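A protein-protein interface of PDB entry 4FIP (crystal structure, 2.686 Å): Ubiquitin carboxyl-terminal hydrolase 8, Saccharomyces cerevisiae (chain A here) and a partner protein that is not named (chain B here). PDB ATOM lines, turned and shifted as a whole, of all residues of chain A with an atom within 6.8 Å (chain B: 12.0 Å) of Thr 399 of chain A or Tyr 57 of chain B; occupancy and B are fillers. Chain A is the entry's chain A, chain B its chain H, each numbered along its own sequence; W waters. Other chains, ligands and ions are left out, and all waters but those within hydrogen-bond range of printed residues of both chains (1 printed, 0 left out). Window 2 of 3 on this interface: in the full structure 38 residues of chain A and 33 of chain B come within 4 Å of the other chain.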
ATOM      1  N   GLU A 289      33.316  24.038 -10.948  1.00  0.00           N
ATOM      2  CA  GLU A 289      34.018  24.908  -9.996  1.00  0.00           C
ATOM      3  C   GLU A 289      35.500  24.557 -10.085  1.00  0.00           C
ATOM      4  O   GLU A 289      35.904  23.403  -9.834  1.00  0.00           O
ATOM      5  CB  GLU A 289      33.524  24.688  -8.561  1.00  0.00           C
ATOM      6  CG  GLU A 289      33.833  25.838  -7.587  1.00  0.00           C
ATOM      7  CD  GLU A 289      34.037  25.376  -6.140  1.00  0.00           C
ATOM      8  OE1 GLU A 289      33.067  25.458  -5.354  1.00  0.00           O
ATOM      9  OE2 GLU A 289      35.160  24.922  -5.786  1.00  0.00           O
ATOM     10  N   ILE A 356      32.029  19.670  -9.508  1.00  0.00           N
ATOM     11  CA  ILE A 356      30.799  20.040 -10.209  1.00  0.00           C
ATOM     12  C   ILE A 356      29.957  20.949  -9.337  1.00  0.00           C
ATOM     13  O   ILE A 356      29.723  20.656  -8.177  1.00  0.00           O
ATOM     14  CB  ILE A 356      29.966  18.837 -10.688  1.00  0.00           C
ATOM     15  CG1 ILE A 356      30.837  17.920 -11.574  1.00  0.00           C
ATOM     16  CG2 ILE A 356      28.746  19.346 -11.454  1.00  0.00           C
ATOM     17  CD1 ILE A 356      30.421  16.464 -11.607  1.00  0.00           C
ATOM     18  N   HIS A 357      29.525  22.058  -9.925  1.00  0.00           N
ATOM     19  CA  HIS A 357      28.721  23.057  -9.245  1.00  0.00           C
ATOM     20  C   HIS A 357      27.271  22.925  -9.633  1.00  0.00           C
ATOM     21  O   HIS A 357      26.402  23.005  -8.816  1.00  0.00           O
ATOM     22  CB  HIS A 357      29.272  24.432  -9.597  1.00  0.00           C
ATOM     23  CG  HIS A 357      28.443  25.583  -9.088  1.00  0.00           C
ATOM     24  ND1 HIS A 357      28.350  25.896  -7.765  1.00  0.00           N
ATOM     25  CD2 HIS A 357      27.687  26.536  -9.778  1.00  0.00           C
ATOM     26  CE1 HIS A 357      27.550  26.976  -7.621  1.00  0.00           C
ATOM     27  NE2 HIS A 357      27.143  27.364  -8.864  1.00  0.00           N
ATOM     28  N   LYS A 358      27.010  22.731 -10.905  1.00  0.00           N
ATOM     29  CA  LYS A 358      25.685  22.409 -11.398  1.00  0.00           C
ATOM     30  C   LYS A 358      25.747  21.198 -12.364  1.00  0.00           C
ATOM     31  O   LYS A 358      26.587  21.147 -13.259  1.00  0.00           O
ATOM     32  CB  LYS A 358      25.110  23.622 -12.115  1.00  0.00           C
ATOM     33  CG  LYS A 358      23.945  24.251 -11.395  1.00  0.00           C
ATOM     34  CD  LYS A 358      24.300  24.845 -10.067  1.00  0.00           C
ATOM     35  CE  LYS A 358      23.225  25.815  -9.595  1.00  0.00           C
ATOM     36  NZ  LYS A 358      22.170  25.114  -8.829  1.00  0.00           N
ATOM     37  N   LEU A 359      24.860  20.235 -12.165  1.00  0.00           N
ATOM     38  CA  LEU A 359      24.740  19.100 -13.064  1.00  0.00           C
ATOM     39  C   LEU A 359      23.753  19.378 -14.190  1.00  0.00           C
ATOM     40  O   LEU A 359      22.818  20.156 -14.008  1.00  0.00           O
ATOM     41  CB  LEU A 359      24.227  17.903 -12.300  1.00  0.00           C
ATOM     42  CG  LEU A 359      25.273  17.113 -11.516  1.00  0.00           C
ATOM     43  CD1 LEU A 359      24.604  16.345 -10.393  1.00  0.00           C
ATOM     44  CD2 LEU A 359      26.033  16.191 -12.457  1.00  0.00           C
ATOM     45  N   PRO A 360      23.924  18.714 -15.350  1.00  0.00           N
ATOM     46  CA  PRO A 360      22.922  18.790 -16.388  1.00  0.00           C
ATOM     47  C   PRO A 360      21.857  17.675 -16.250  1.00  0.00           C
ATOM     48  O   PRO A 360      22.082  16.624 -15.562  1.00  0.00           O
ATOM     49  CB  PRO A 360      23.750  18.572 -17.646  1.00  0.00           C
ATOM     50  CG  PRO A 360      24.837  17.648 -17.225  1.00  0.00           C
ATOM     51  CD  PRO A 360      25.008  17.801 -15.741  1.00  0.00           C
ATOM     52  N   CYS A 397      30.640  16.427  -6.776  1.00  0.00           N
ATOM     53  CA  CYS A 397      30.027  17.731  -6.562  1.00  0.00           C
ATOM     54  C   CYS A 397      30.633  18.432  -5.357  1.00  0.00           C
ATOM     55  O   CYS A 397      30.943  17.772  -4.385  1.00  0.00           O
ATOM     56  CB  CYS A 397      28.526  17.556  -6.295  1.00  0.00           C
ATOM     57  SG  CYS A 397      27.584  16.745  -7.612  1.00  0.00           S
ATOM     58  N   SER A 398      30.755  19.762  -5.399  1.00  0.00           N
ATOM     59  CA  SER A 398      31.219  20.575  -4.257  1.00  0.00           C
ATOM     60  C   SER A 398      30.077  20.768  -3.251  1.00  0.00           C
ATOM     61  O   SER A 398      28.993  20.268  -3.491  1.00  0.00           O
ATOM     62  CB  SER A 398      31.704  21.944  -4.743  1.00  0.00           C
ATOM     63  OG  SER A 398      32.086  21.927  -6.104  1.00  0.00           O
ATOM     64  N   THR A 399      30.298  21.509  -2.156  1.00  0.00           N
ATOM     65  CA  THR A 399      29.297  21.671  -1.036  1.00  0.00           C
ATOM     66  C   THR A 399      27.808  21.630  -1.456  1.00  0.00           C
ATOM     67  O   THR A 399      26.915  21.323  -0.653  1.00  0.00           O
ATOM     68  CB  THR A 399      29.528  22.992  -0.210  1.00  0.00           C
ATOM     69  OG1 THR A 399      30.932  23.263  -0.050  1.00  0.00           O
ATOM     70  CG2 THR A 399      28.852  22.923   1.198  1.00  0.00           C
ATOM     71  N   GLU A 407      29.874  20.668   8.344  1.00  0.00           N
ATOM     72  CA  GLU A 407      28.399  20.741   8.404  1.00  0.00           C
ATOM     73  C   GLU A 407      27.808  19.701   7.453  1.00  0.00           C
ATOM     74  O   GLU A 407      28.413  19.396   6.420  1.00  0.00           O
ATOM     75  CB  GLU A 407      27.911  22.148   8.000  1.00  0.00           C
ATOM     76  CG  GLU A 407      26.392  22.343   7.953  1.00  0.00           C
ATOM     77  CD  GLU A 407      25.751  22.361   9.332  1.00  0.00           C
ATOM     78  OE1 GLU A 407      26.179  23.182  10.172  1.00  0.00           O
ATOM     79  OE2 GLU A 407      24.813  21.570   9.579  1.00  0.00           O
ATOM     80  N   GLY A 409      26.241  19.168   4.715  1.00  0.00           N
ATOM     81  CA  GLY A 409      25.900  19.338   3.307  1.00  0.00           C
ATOM     82  C   GLY A 409      26.591  18.203   2.560  1.00  0.00           C
ATOM     83  O   GLY A 409      27.172  18.417   1.486  1.00  0.00           O
ATOM     84  N   LYS A 410      26.555  17.005   3.165  1.00  0.00           N
ATOM     85  CA  LYS A 410      27.003  15.764   2.532  1.00  0.00           C
ATOM     86  C   LYS A 410      26.065  15.459   1.393  1.00  0.00           C
ATOM     87  O   LYS A 410      24.853  15.481   1.571  1.00  0.00           O
ATOM     88  CB  LYS A 410      26.973  14.600   3.518  1.00  0.00           C
ATOM     89  CG  LYS A 410      27.271  13.246   2.889  1.00  0.00           C
ATOM     90  CD  LYS A 410      28.145  12.383   3.797  1.00  0.00           C
ATOM     91  CE  LYS A 410      27.387  11.832   5.004  1.00  0.00           C
ATOM     92  NZ  LYS A 410      26.581  10.619   4.670  1.00  0.00           N
ATOM     93  N   VAL A 411      26.626  15.175   0.227  1.00  0.00           N
ATOM     94  CA  VAL A 411      25.861  15.188  -1.013  1.00  0.00           C
ATOM     95  C   VAL A 411      25.008  13.923  -1.133  1.00  0.00           C
ATOM     96  O   VAL A 411      25.517  12.807  -0.995  1.00  0.00           O
ATOM     97  CB  VAL A 411      26.799  15.324  -2.234  1.00  0.00           C
ATOM     98  CG1 VAL A 411      25.992  15.409  -3.511  1.00  0.00           C
ATOM     99  CG2 VAL A 411      27.683  16.556  -2.085  1.00  0.00           C
ATOM    100  N   PRO A 412      23.703  14.092  -1.396  1.00  0.00           N
ATOM    101  CA  PRO A 412      22.767  12.960  -1.547  1.00  0.00           C
ATOM    102  C   PRO A 412      22.961  12.214  -2.854  1.00  0.00           C
ATOM    103  O   PRO A 412      23.624  12.714  -3.745  1.00  0.00           O
ATOM    104  CB  PRO A 412      21.408  13.646  -1.590  1.00  0.00           C
ATOM    105  CG  PRO A 412      21.699  14.972  -2.245  1.00  0.00           C
ATOM    106  CD  PRO A 412      23.082  15.376  -1.793  1.00  0.00           C
ATOM    107  N   ILE A 414      22.678  11.142  -6.497  1.00  0.00           N
ATOM    108  CA  ILE A 414      22.191  11.763  -7.715  1.00  0.00           C
ATOM    109  C   ILE A 414      22.507  10.787  -8.843  1.00  0.00           C
ATOM    110  O   ILE A 414      23.626  10.743  -9.359  1.00  0.00           O
ATOM    111  CB  ILE A 414      22.885  13.125  -7.984  1.00  0.00           C
ATOM    112  CG1 ILE A 414      22.692  14.053  -6.797  1.00  0.00           C
ATOM    113  CG2 ILE A 414      22.365  13.777  -9.261  1.00  0.00           C
ATOM    114  CD1 ILE A 414      23.421  15.371  -6.918  1.00  0.00           C
ATOM    115  N   TYR A 416      22.118   8.892 -12.449  1.00  0.00           N
ATOM    116  CA  TYR A 416      21.784   8.916 -13.868  1.00  0.00           C
ATOM    117  C   TYR A 416      21.645   7.512 -14.418  1.00  0.00           C
ATOM    118  O   TYR A 416      22.210   6.601 -13.858  1.00  0.00           O
ATOM    119  CB  TYR A 416      22.945   9.543 -14.611  1.00  0.00           C
ATOM    120  CG  TYR A 416      23.062  11.017 -14.449  1.00  0.00           C
ATOM    121  CD1 TYR A 416      23.717  11.566 -13.360  1.00  0.00           C
ATOM    122  CD2 TYR A 416      22.541  11.870 -15.418  1.00  0.00           C
ATOM    123  CE1 TYR A 416      23.821  12.925 -13.237  1.00  0.00           C
ATOM    124  CE2 TYR A 416      22.647  13.230 -15.299  1.00  0.00           C
ATOM    125  CZ  TYR A 416      23.277  13.746 -14.194  1.00  0.00           C
ATOM    126  OH  TYR A 416      23.364  15.106 -14.092  1.00  0.00           O
ATOM    127  N   VAL A 475      17.259  11.747  -7.843  1.00  0.00           N
ATOM    128  CA  VAL A 475      18.014  12.634  -6.969  1.00  0.00           C
ATOM    129  C   VAL A 475      17.338  12.730  -5.612  1.00  0.00           C
ATOM    130  O   VAL A 475      16.188  13.127  -5.509  1.00  0.00           O
ATOM    131  CB  VAL A 475      18.296  14.010  -7.645  1.00  0.00           C
ATOM    132  CG1 VAL A 475      17.381  14.262  -8.809  1.00  0.00           C
ATOM    133  CG2 VAL A 475      18.287  15.165  -6.672  1.00  0.00           C
ATOM    134  N   ASN A 476      18.056  12.322  -4.572  1.00  0.00           N
ATOM    135  CA  ASN A 476      17.535  12.348  -3.200  1.00  0.00           C
ATOM    136  C   ASN A 476      17.769  13.690  -2.477  1.00  0.00           C
ATOM    137  O   ASN A 476      18.128  14.698  -3.087  1.00  0.00           O
ATOM    138  CB  ASN A 476      18.136  11.208  -2.401  1.00  0.00           C
ATOM    139  CG  ASN A 476      17.695   9.873  -2.909  1.00  0.00           C
ATOM    140  OD1 ASN A 476      16.691   9.764  -3.626  1.00  0.00           O
ATOM    141  ND2 ASN A 476      18.430   8.840  -2.546  1.00  0.00           N
ATOM    142  OXT ASN A 476      17.581  13.841  -1.266  1.00  0.00           O
ATOM    143  N   HIS B  48      10.616  11.120  -7.432  1.00  0.00           N
ATOM    144  CA  HIS B  48      11.888  10.742  -6.894  1.00  0.00           C
ATOM    145  C   HIS B  48      13.037  11.532  -7.448  1.00  0.00           C
ATOM    146  O   HIS B  48      14.111  11.015  -7.803  1.00  0.00           O
ATOM    147  CB  HIS B  48      12.073   9.240  -6.995  1.00  0.00           C
ATOM    148  CG  HIS B  48      11.767   8.695  -8.333  1.00  0.00           C
ATOM    149  ND1 HIS B  48      12.509   9.003  -9.409  1.00  0.00           N
ATOM    150  CD2 HIS B  48      10.774   7.818  -8.763  1.00  0.00           C
ATOM    151  CE1 HIS B  48      12.011   8.364 -10.485  1.00  0.00           C
ATOM    152  NE2 HIS B  48      10.944   7.635 -10.087  1.00  0.00           N
ATOM    153  N   MET B  49      12.806  12.832  -7.458  1.00  0.00           N
ATOM    154  CA  MET B  49      13.838  13.806  -7.625  1.00  0.00           C
ATOM    155  C   MET B  49      13.446  14.909  -6.690  1.00  0.00           C
ATOM    156  O   MET B  49      12.614  15.726  -7.009  1.00  0.00           O
ATOM    157  CB  MET B  49      13.879  14.309  -9.062  1.00  0.00           C
ATOM    158  CG  MET B  49      14.009  13.196 -10.100  1.00  0.00           C
ATOM    159  SD  MET B  49      14.500  13.833 -11.708  1.00  0.00           S
ATOM    160  CE  MET B  49      12.959  14.400 -12.427  1.00  0.00           C
ATOM    161  N   ASN B  50      14.023  14.887  -5.507  1.00  0.00           N
ATOM    162  CA  ASN B  50      13.749  15.866  -4.457  1.00  0.00           C
ATOM    163  C   ASN B  50      13.936  17.342  -4.850  1.00  0.00           C
ATOM    164  O   ASN B  50      15.008  17.762  -5.291  1.00  0.00           O
ATOM    165  CB  ASN B  50      14.634  15.521  -3.258  1.00  0.00           C
ATOM    166  CG  ASN B  50      14.610  16.579  -2.202  1.00  0.00           C
ATOM    167  OD1 ASN B  50      15.445  17.509  -2.190  1.00  0.00           O
ATOM    168  ND2 ASN B  50      13.645  16.474  -1.318  1.00  0.00           N
ATOM    169  N   ARG B  51      12.898  18.135  -4.645  1.00  0.00           N
ATOM    170  CA  ARG B  51      12.909  19.533  -5.071  1.00  0.00           C
ATOM    171  C   ARG B  51      14.025  20.423  -4.466  1.00  0.00           C
ATOM    172  O   ARG B  51      14.439  21.412  -5.091  1.00  0.00           O
ATOM    173  CB  ARG B  51      11.541  20.158  -4.807  1.00  0.00           C
ATOM    174  CG  ARG B  51      11.426  21.585  -5.304  1.00  0.00           C
ATOM    175  CD  ARG B  51       9.984  22.024  -5.416  1.00  0.00           C
ATOM    176  NE  ARG B  51       9.888  23.380  -5.949  1.00  0.00           N
ATOM    177  CZ  ARG B  51       9.853  23.691  -7.248  1.00  0.00           C
ATOM    178  NH1 ARG B  51       9.897  22.746  -8.181  1.00  0.00           N
ATOM    179  NH2 ARG B  51       9.756  24.955  -7.626  1.00  0.00           N
ATOM    180  N   GLU B  52      14.526  20.097  -3.280  1.00  0.00           N
ATOM    181  CA  GLU B  52      15.611  20.915  -2.701  1.00  0.00           C
ATOM    182  C   GLU B  52      16.950  20.581  -3.355  1.00  0.00           C
ATOM    183  O   GLU B  52      17.706  21.466  -3.722  1.00  0.00           O
ATOM    184  CB  GLU B  52      15.688  20.797  -1.169  1.00  0.00           C
ATOM    185  CG  GLU B  52      14.574  21.553  -0.433  1.00  0.00           C
ATOM    186  CD  GLU B  52      13.189  20.908  -0.543  1.00  0.00           C
ATOM    187  OE1 GLU B  52      13.102  19.655  -0.403  1.00  0.00           O
ATOM    188  OE2 GLU B  52      12.181  21.654  -0.760  1.00  0.00           O
ATOM    189  N   SER B  53      17.230  19.300  -3.533  1.00  0.00           N
ATOM    190  CA  SER B  53      18.451  18.879  -4.222  1.00  0.00           C
ATOM    191  C   SER B  53      18.528  19.347  -5.685  1.00  0.00           C
ATOM    192  O   SER B  53      19.605  19.761  -6.146  1.00  0.00           O
ATOM    193  CB  SER B  53      18.565  17.370  -4.124  1.00  0.00           C
ATOM    194  OG  SER B  53      18.724  17.001  -2.750  1.00  0.00           O
ATOM    195  N   LEU B  54      17.385  19.298  -6.389  1.00  0.00           N
ATOM    196  CA  LEU B  54      17.243  19.884  -7.724  1.00  0.00           C
ATOM    197  C   LEU B  54      17.565  21.361  -7.742  1.00  0.00           C
ATOM    198  O   LEU B  54      18.410  21.795  -8.529  1.00  0.00           O
ATOM    199  CB  LEU B  54      15.837  19.701  -8.242  1.00  0.00           C
ATOM    200  CG  LEU B  54      15.413  18.277  -8.620  1.00  0.00           C
ATOM    201  CD1 LEU B  54      13.921  18.272  -8.937  1.00  0.00           C
ATOM    202  CD2 LEU B  54      16.190  17.729  -9.810  1.00  0.00           C
ATOM    203  N   LYS B  55      16.888  22.130  -6.880  1.00  0.00           N
ATOM    204  CA  LYS B  55      17.152  23.575  -6.694  1.00  0.00           C
ATOM    205  C   LYS B  55      18.650  23.846  -6.461  1.00  0.00           C
ATOM    206  O   LYS B  55      19.198  24.818  -6.968  1.00  0.00           O
ATOM    207  CB  LYS B  55      16.344  24.140  -5.501  1.00  0.00           C
ATOM    208  CG  LYS B  55      14.893  24.576  -5.780  1.00  0.00           C
ATOM    209  CD  LYS B  55      14.078  24.777  -4.497  1.00  0.00           C
ATOM    210  CE  LYS B  55      13.268  26.082  -4.462  1.00  0.00           C
ATOM    211  NZ  LYS B  55      11.771  25.958  -4.541  1.00  0.00           N
ATOM    212  N   LYS B  56      19.293  22.945  -5.717  1.00  0.00           N
ATOM    213  CA  LYS B  56      20.674  23.087  -5.244  1.00  0.00           C
ATOM    214  C   LYS B  56      21.716  22.640  -6.288  1.00  0.00           C
ATOM    215  O   LYS B  56      22.556  23.432  -6.681  1.00  0.00           O
ATOM    216  CB  LYS B  56      20.797  22.275  -3.945  1.00  0.00           C
ATOM    217  CG  LYS B  56      21.883  22.684  -2.969  1.00  0.00           C
ATOM    218  CD  LYS B  56      21.418  22.714  -1.492  1.00  0.00           C
ATOM    219  CE  LYS B  56      22.618  23.054  -0.576  1.00  0.00           C
ATOM    220  NZ  LYS B  56      22.317  23.710   0.733  1.00  0.00           N
ATOM    221  N   TYR B  57      21.625  21.393  -6.763  1.00  0.00           N
ATOM    222  CA  TYR B  57      22.638  20.814  -7.648  1.00  0.00           C
ATOM    223  C   TYR B  57      22.270  20.822  -9.123  1.00  0.00           C
ATOM    224  O   TYR B  57      23.047  20.344  -9.953  1.00  0.00           O
ATOM    225  CB  TYR B  57      22.923  19.374  -7.251  1.00  0.00           C
ATOM    226  CG  TYR B  57      23.275  19.207  -5.805  1.00  0.00           C
ATOM    227  CD1 TYR B  57      24.505  19.589  -5.335  1.00  0.00           C
ATOM    228  CD2 TYR B  57      22.350  18.678  -4.889  1.00  0.00           C
ATOM    229  CE1 TYR B  57      24.829  19.450  -3.991  1.00  0.00           C
ATOM    230  CE2 TYR B  57      22.667  18.539  -3.544  1.00  0.00           C
ATOM    231  CZ  TYR B  57      23.906  18.923  -3.100  1.00  0.00           C
ATOM    232  OH  TYR B  57      24.237  18.779  -1.782  1.00  0.00           O
ATOM    233  N   PHE B  58      21.094  21.327  -9.476  1.00  0.00           N
ATOM    234  CA  PHE B  58      20.726  21.410 -10.889  1.00  0.00           C
ATOM    235  C   PHE B  58      20.479  22.875 -11.197  1.00  0.00           C
ATOM    236  O   PHE B  58      20.431  23.666 -10.296  1.00  0.00           O
ATOM    237  CB  PHE B  58      19.543  20.452 -11.209  1.00  0.00           C
ATOM    238  CG  PHE B  58      19.951  18.988 -11.229  1.00  0.00           C
ATOM    239  CD1 PHE B  58      20.280  18.322 -10.062  1.00  0.00           C
ATOM    240  CD2 PHE B  58      20.074  18.297 -12.412  1.00  0.00           C
ATOM    241  CE1 PHE B  58      20.712  16.992 -10.075  1.00  0.00           C
ATOM    242  CE2 PHE B  58      20.503  16.974 -12.433  1.00  0.00           C
ATOM    243  CZ  PHE B  58      20.820  16.324 -11.262  1.00  0.00           C
ATOM    244  N   ASN B  59      20.411  23.249 -12.459  1.00  0.00           N
ATOM    245  CA  ASN B  59      20.124  24.632 -12.838  1.00  0.00           C
ATOM    246  C   ASN B  59      18.646  25.066 -12.602  1.00  0.00           C
ATOM    247  O   ASN B  59      17.718  24.266 -12.710  1.00  0.00           O
ATOM    248  CB  ASN B  59      20.482  24.860 -14.330  1.00  0.00           C
ATOM    249  CG  ASN B  59      21.986  24.989 -14.589  1.00  0.00           C
ATOM    250  OD1 ASN B  59      22.649  25.926 -14.120  1.00  0.00           O
ATOM    251  ND2 ASN B  59      22.519  24.068 -15.375  1.00  0.00           N
ATOM    252  N   PRO B  60      18.417  26.363 -12.332  1.00  0.00           N
ATOM    253  CA  PRO B  60      17.033  26.837 -12.092  1.00  0.00           C
ATOM    254  C   PRO B  60      16.056  26.620 -13.253  1.00  0.00           C
ATOM    255  O   PRO B  60      14.878  26.524 -12.990  1.00  0.00           O
ATOM    256  CB  PRO B  60      17.202  28.332 -11.827  1.00  0.00           C
ATOM    257  CG  PRO B  60      18.517  28.701 -12.442  1.00  0.00           C
ATOM    258  CD  PRO B  60      19.387  27.475 -12.396  1.00  0.00           C
ATOM    259  N   ASN B  61      16.549  26.541 -14.502  1.00  0.00           N
ATOM    260  CA  ASN B  61      15.727  26.333 -15.740  1.00  0.00           C
ATOM    261  C   ASN B  61      15.740  24.882 -16.314  1.00  0.00           C
ATOM    262  O   ASN B  61      15.231  24.624 -17.399  1.00  0.00           O
ATOM    263  CB  ASN B  61      16.079  27.349 -16.870  1.00  0.00           C
ATOM    264  CG  ASN B  61      17.542  27.852 -16.850  1.00  0.00           C
ATOM    265  OD1 ASN B  61      18.031  28.337 -15.830  1.00  0.00           O
ATOM    266  ND2 ASN B  61      18.211  27.823 -18.009  1.00  0.00           N
ATOM    267  N   ALA B  62      16.322  23.945 -15.564  1.00  0.00           N
ATOM    268  CA  ALA B  62      16.540  22.584 -16.017  1.00  0.00           C
ATOM    269  C   ALA B  62      15.274  21.998 -16.578  1.00  0.00           C
ATOM    270  O   ALA B  62      14.234  22.163 -16.014  1.00  0.00           O
ATOM    271  CB  ALA B  62      16.984  21.752 -14.833  1.00  0.00           C
ATOM    272  N   GLN B  63      15.335  21.299 -17.684  1.00  0.00           N
ATOM    273  CA  GLN B  63      14.188  20.532 -18.098  1.00  0.00           C
ATOM    274  C   GLN B  63      14.321  19.210 -17.418  1.00  0.00           C
ATOM    275  O   GLN B  63      15.420  18.726 -17.262  1.00  0.00           O
ATOM    276  CB  GLN B  63      14.177  20.293 -19.601  1.00  0.00           C
ATOM    277  CG  GLN B  63      13.995  21.541 -20.436  1.00  0.00           C
ATOM    278  CD  GLN B  63      13.514  21.236 -21.855  1.00  0.00           C
ATOM    279  OE1 GLN B  63      12.970  20.165 -22.125  1.00  0.00           O
ATOM    280  NE2 GLN B  63      13.727  22.173 -22.764  1.00  0.00           N
ATOM    281  N   LEU B  64      13.218  18.587 -17.046  1.00  0.00           N
ATOM    282  CA  LEU B  64      13.295  17.249 -16.463  1.00  0.00           C
ATOM    283  C   LEU B  64      12.155  16.374 -16.934  1.00  0.00           C
ATOM    284  O   LEU B  64      11.035  16.850 -17.047  1.00  0.00           O
ATOM    285  CB  LEU B  64      13.253  17.347 -14.955  1.00  0.00           C
ATOM    286  CG  LEU B  64      14.375  18.166 -14.334  1.00  0.00           C
ATOM    287  CD1 LEU B  64      13.951  18.686 -12.962  1.00  0.00           C
ATOM    288  CD2 LEU B  64      15.643  17.325 -14.297  1.00  0.00           C
HETATM  289  O   HOH W   1      20.643  21.613 -14.851  1.00  0.00           O
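The side-chain amide oxygen (OD1) of Asn 50 of chain B is in hydrogen-bond range of the backbone NH (N) of Glu 52 of chain B (3.0 Å).
OD1 of Asn 50 of chain B lies within hydrogen-bond range of N of Ser 53 of chain B (2.9 Å).
O of Pro 360 of chain A sits at hydrogen-bond distance from OH of Tyr 416 of chain A.
Water W1 bridges O of Leu 359 of chain A (2.8 Å) and N of Asn 59 of chain B (2.9 Å).
O of Asn 476 of chain A sits at hydrogen-bond distance from OG of Ser 53 of chain B (2.4 Å).
The backbone carbonyl oxygen of Val 475 of chain A lies within hydrogen-bond range of the backbone NH of Asn 50 of chain B, 2.8 Å away.
The backbone carbonyl oxygen of Phe 58 of chain B lies within hydrogen-bond range of the side-chain amino group of Lys 358 of chain A (2.7 Å).
N of Val 475 of chain A lies within hydrogen-bond range of O of His 48 of chain B, at 3.2 Å.
O of Lys 56 of chain B is in hydrogen-bond range of NZ of Lys 358 of chain A, at 2.8 Å.
N of Leu 359 of chain A sits at hydrogen-bond distance from O of Tyr 57 of chain B.
Of the 17 printed residues of chain B, 10 touch a printed residue of chain A.
Along chain B the printed residues that touch a printed residue of chain A span positions 48 to 59.
Of the 18 printed residues of chain A, 9 touch a printed residue of chain B.
Hydrophobic or aromatic side chains of chain A that line the printed part of chain B: Leu 359, Pro 412, Ile 414, Tyr 416 and Val 475.
Lys 358 of chain A touches Asn 59 of chain B.
Leu 359 of chain A touches Phe 58 of chain B (O to CD2, 3.7 Å).
Phe 58 of chain B touches Pro 360 of chain A.
Thr 399 of chain A touches Tyr 57 of chain B (O to OH, 3.9 Å).
Ser 53 of chain B touches Pro 412 of chain A (OG to CG, 3.6 Å).
Phe 58 of chain B touches Ile 414 of chain A.
CE2 of Phe 58 of chain B touches OH of Tyr 416 of chain A, at 3.8 Å.
Val 475 of chain A touches Met 49 of chain B.
CG2 of Val 475 of chain A touches CB of Ser 53 of chain B, 3.4 Å away.
CG1 of Val 475 of chain A touches CD2 of Leu 54 of chain B, 3.8 Å away.
Of chain B, only Tyr 57 comes within 4 Å of Thr 399 of chain A.
Printed residues of chain A within 4 Å of Tyr 57 of chain B: Lys 358, Leu 359, Thr 399, Pro 412 and Ile 414.
Printed residues of chain B within 4 Å of Lys 358 of chain A: Lys 55, Lys 56, Tyr 57, Phe 58 and Asn 59.
Of chain B, only Tyr 57 (2.9 Å) and Phe 58 (3.7 Å) come within 4 Å of Leu 359 of chain A.
No residue of chain B comes within 4 Å of Cys 397 of chain A.
No residue of chain B comes within 4 Å of Ser 398 of chain A.
Pro 412 of chain A touches just these residues of chain B: Ser 53 and Tyr 57.
Of the printed residues of chain A, Leu 54 of chain B touches Val 475 (3.8 Å).
Printed residues of chain B within 4 Å of Val 475 of chain A: His 48, Met 49, Asn 50, Ser 53 and Leu 54.
Of the printed residues of chain B, Asn 476 of chain A touches Asn 50 (3.6 Å) and Ser 53 (2.4 Å).
Ala 62 of chain B touches none of the printed residues of chain A.
Glu 289 of chain A touches none of the printed residues of chain B.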
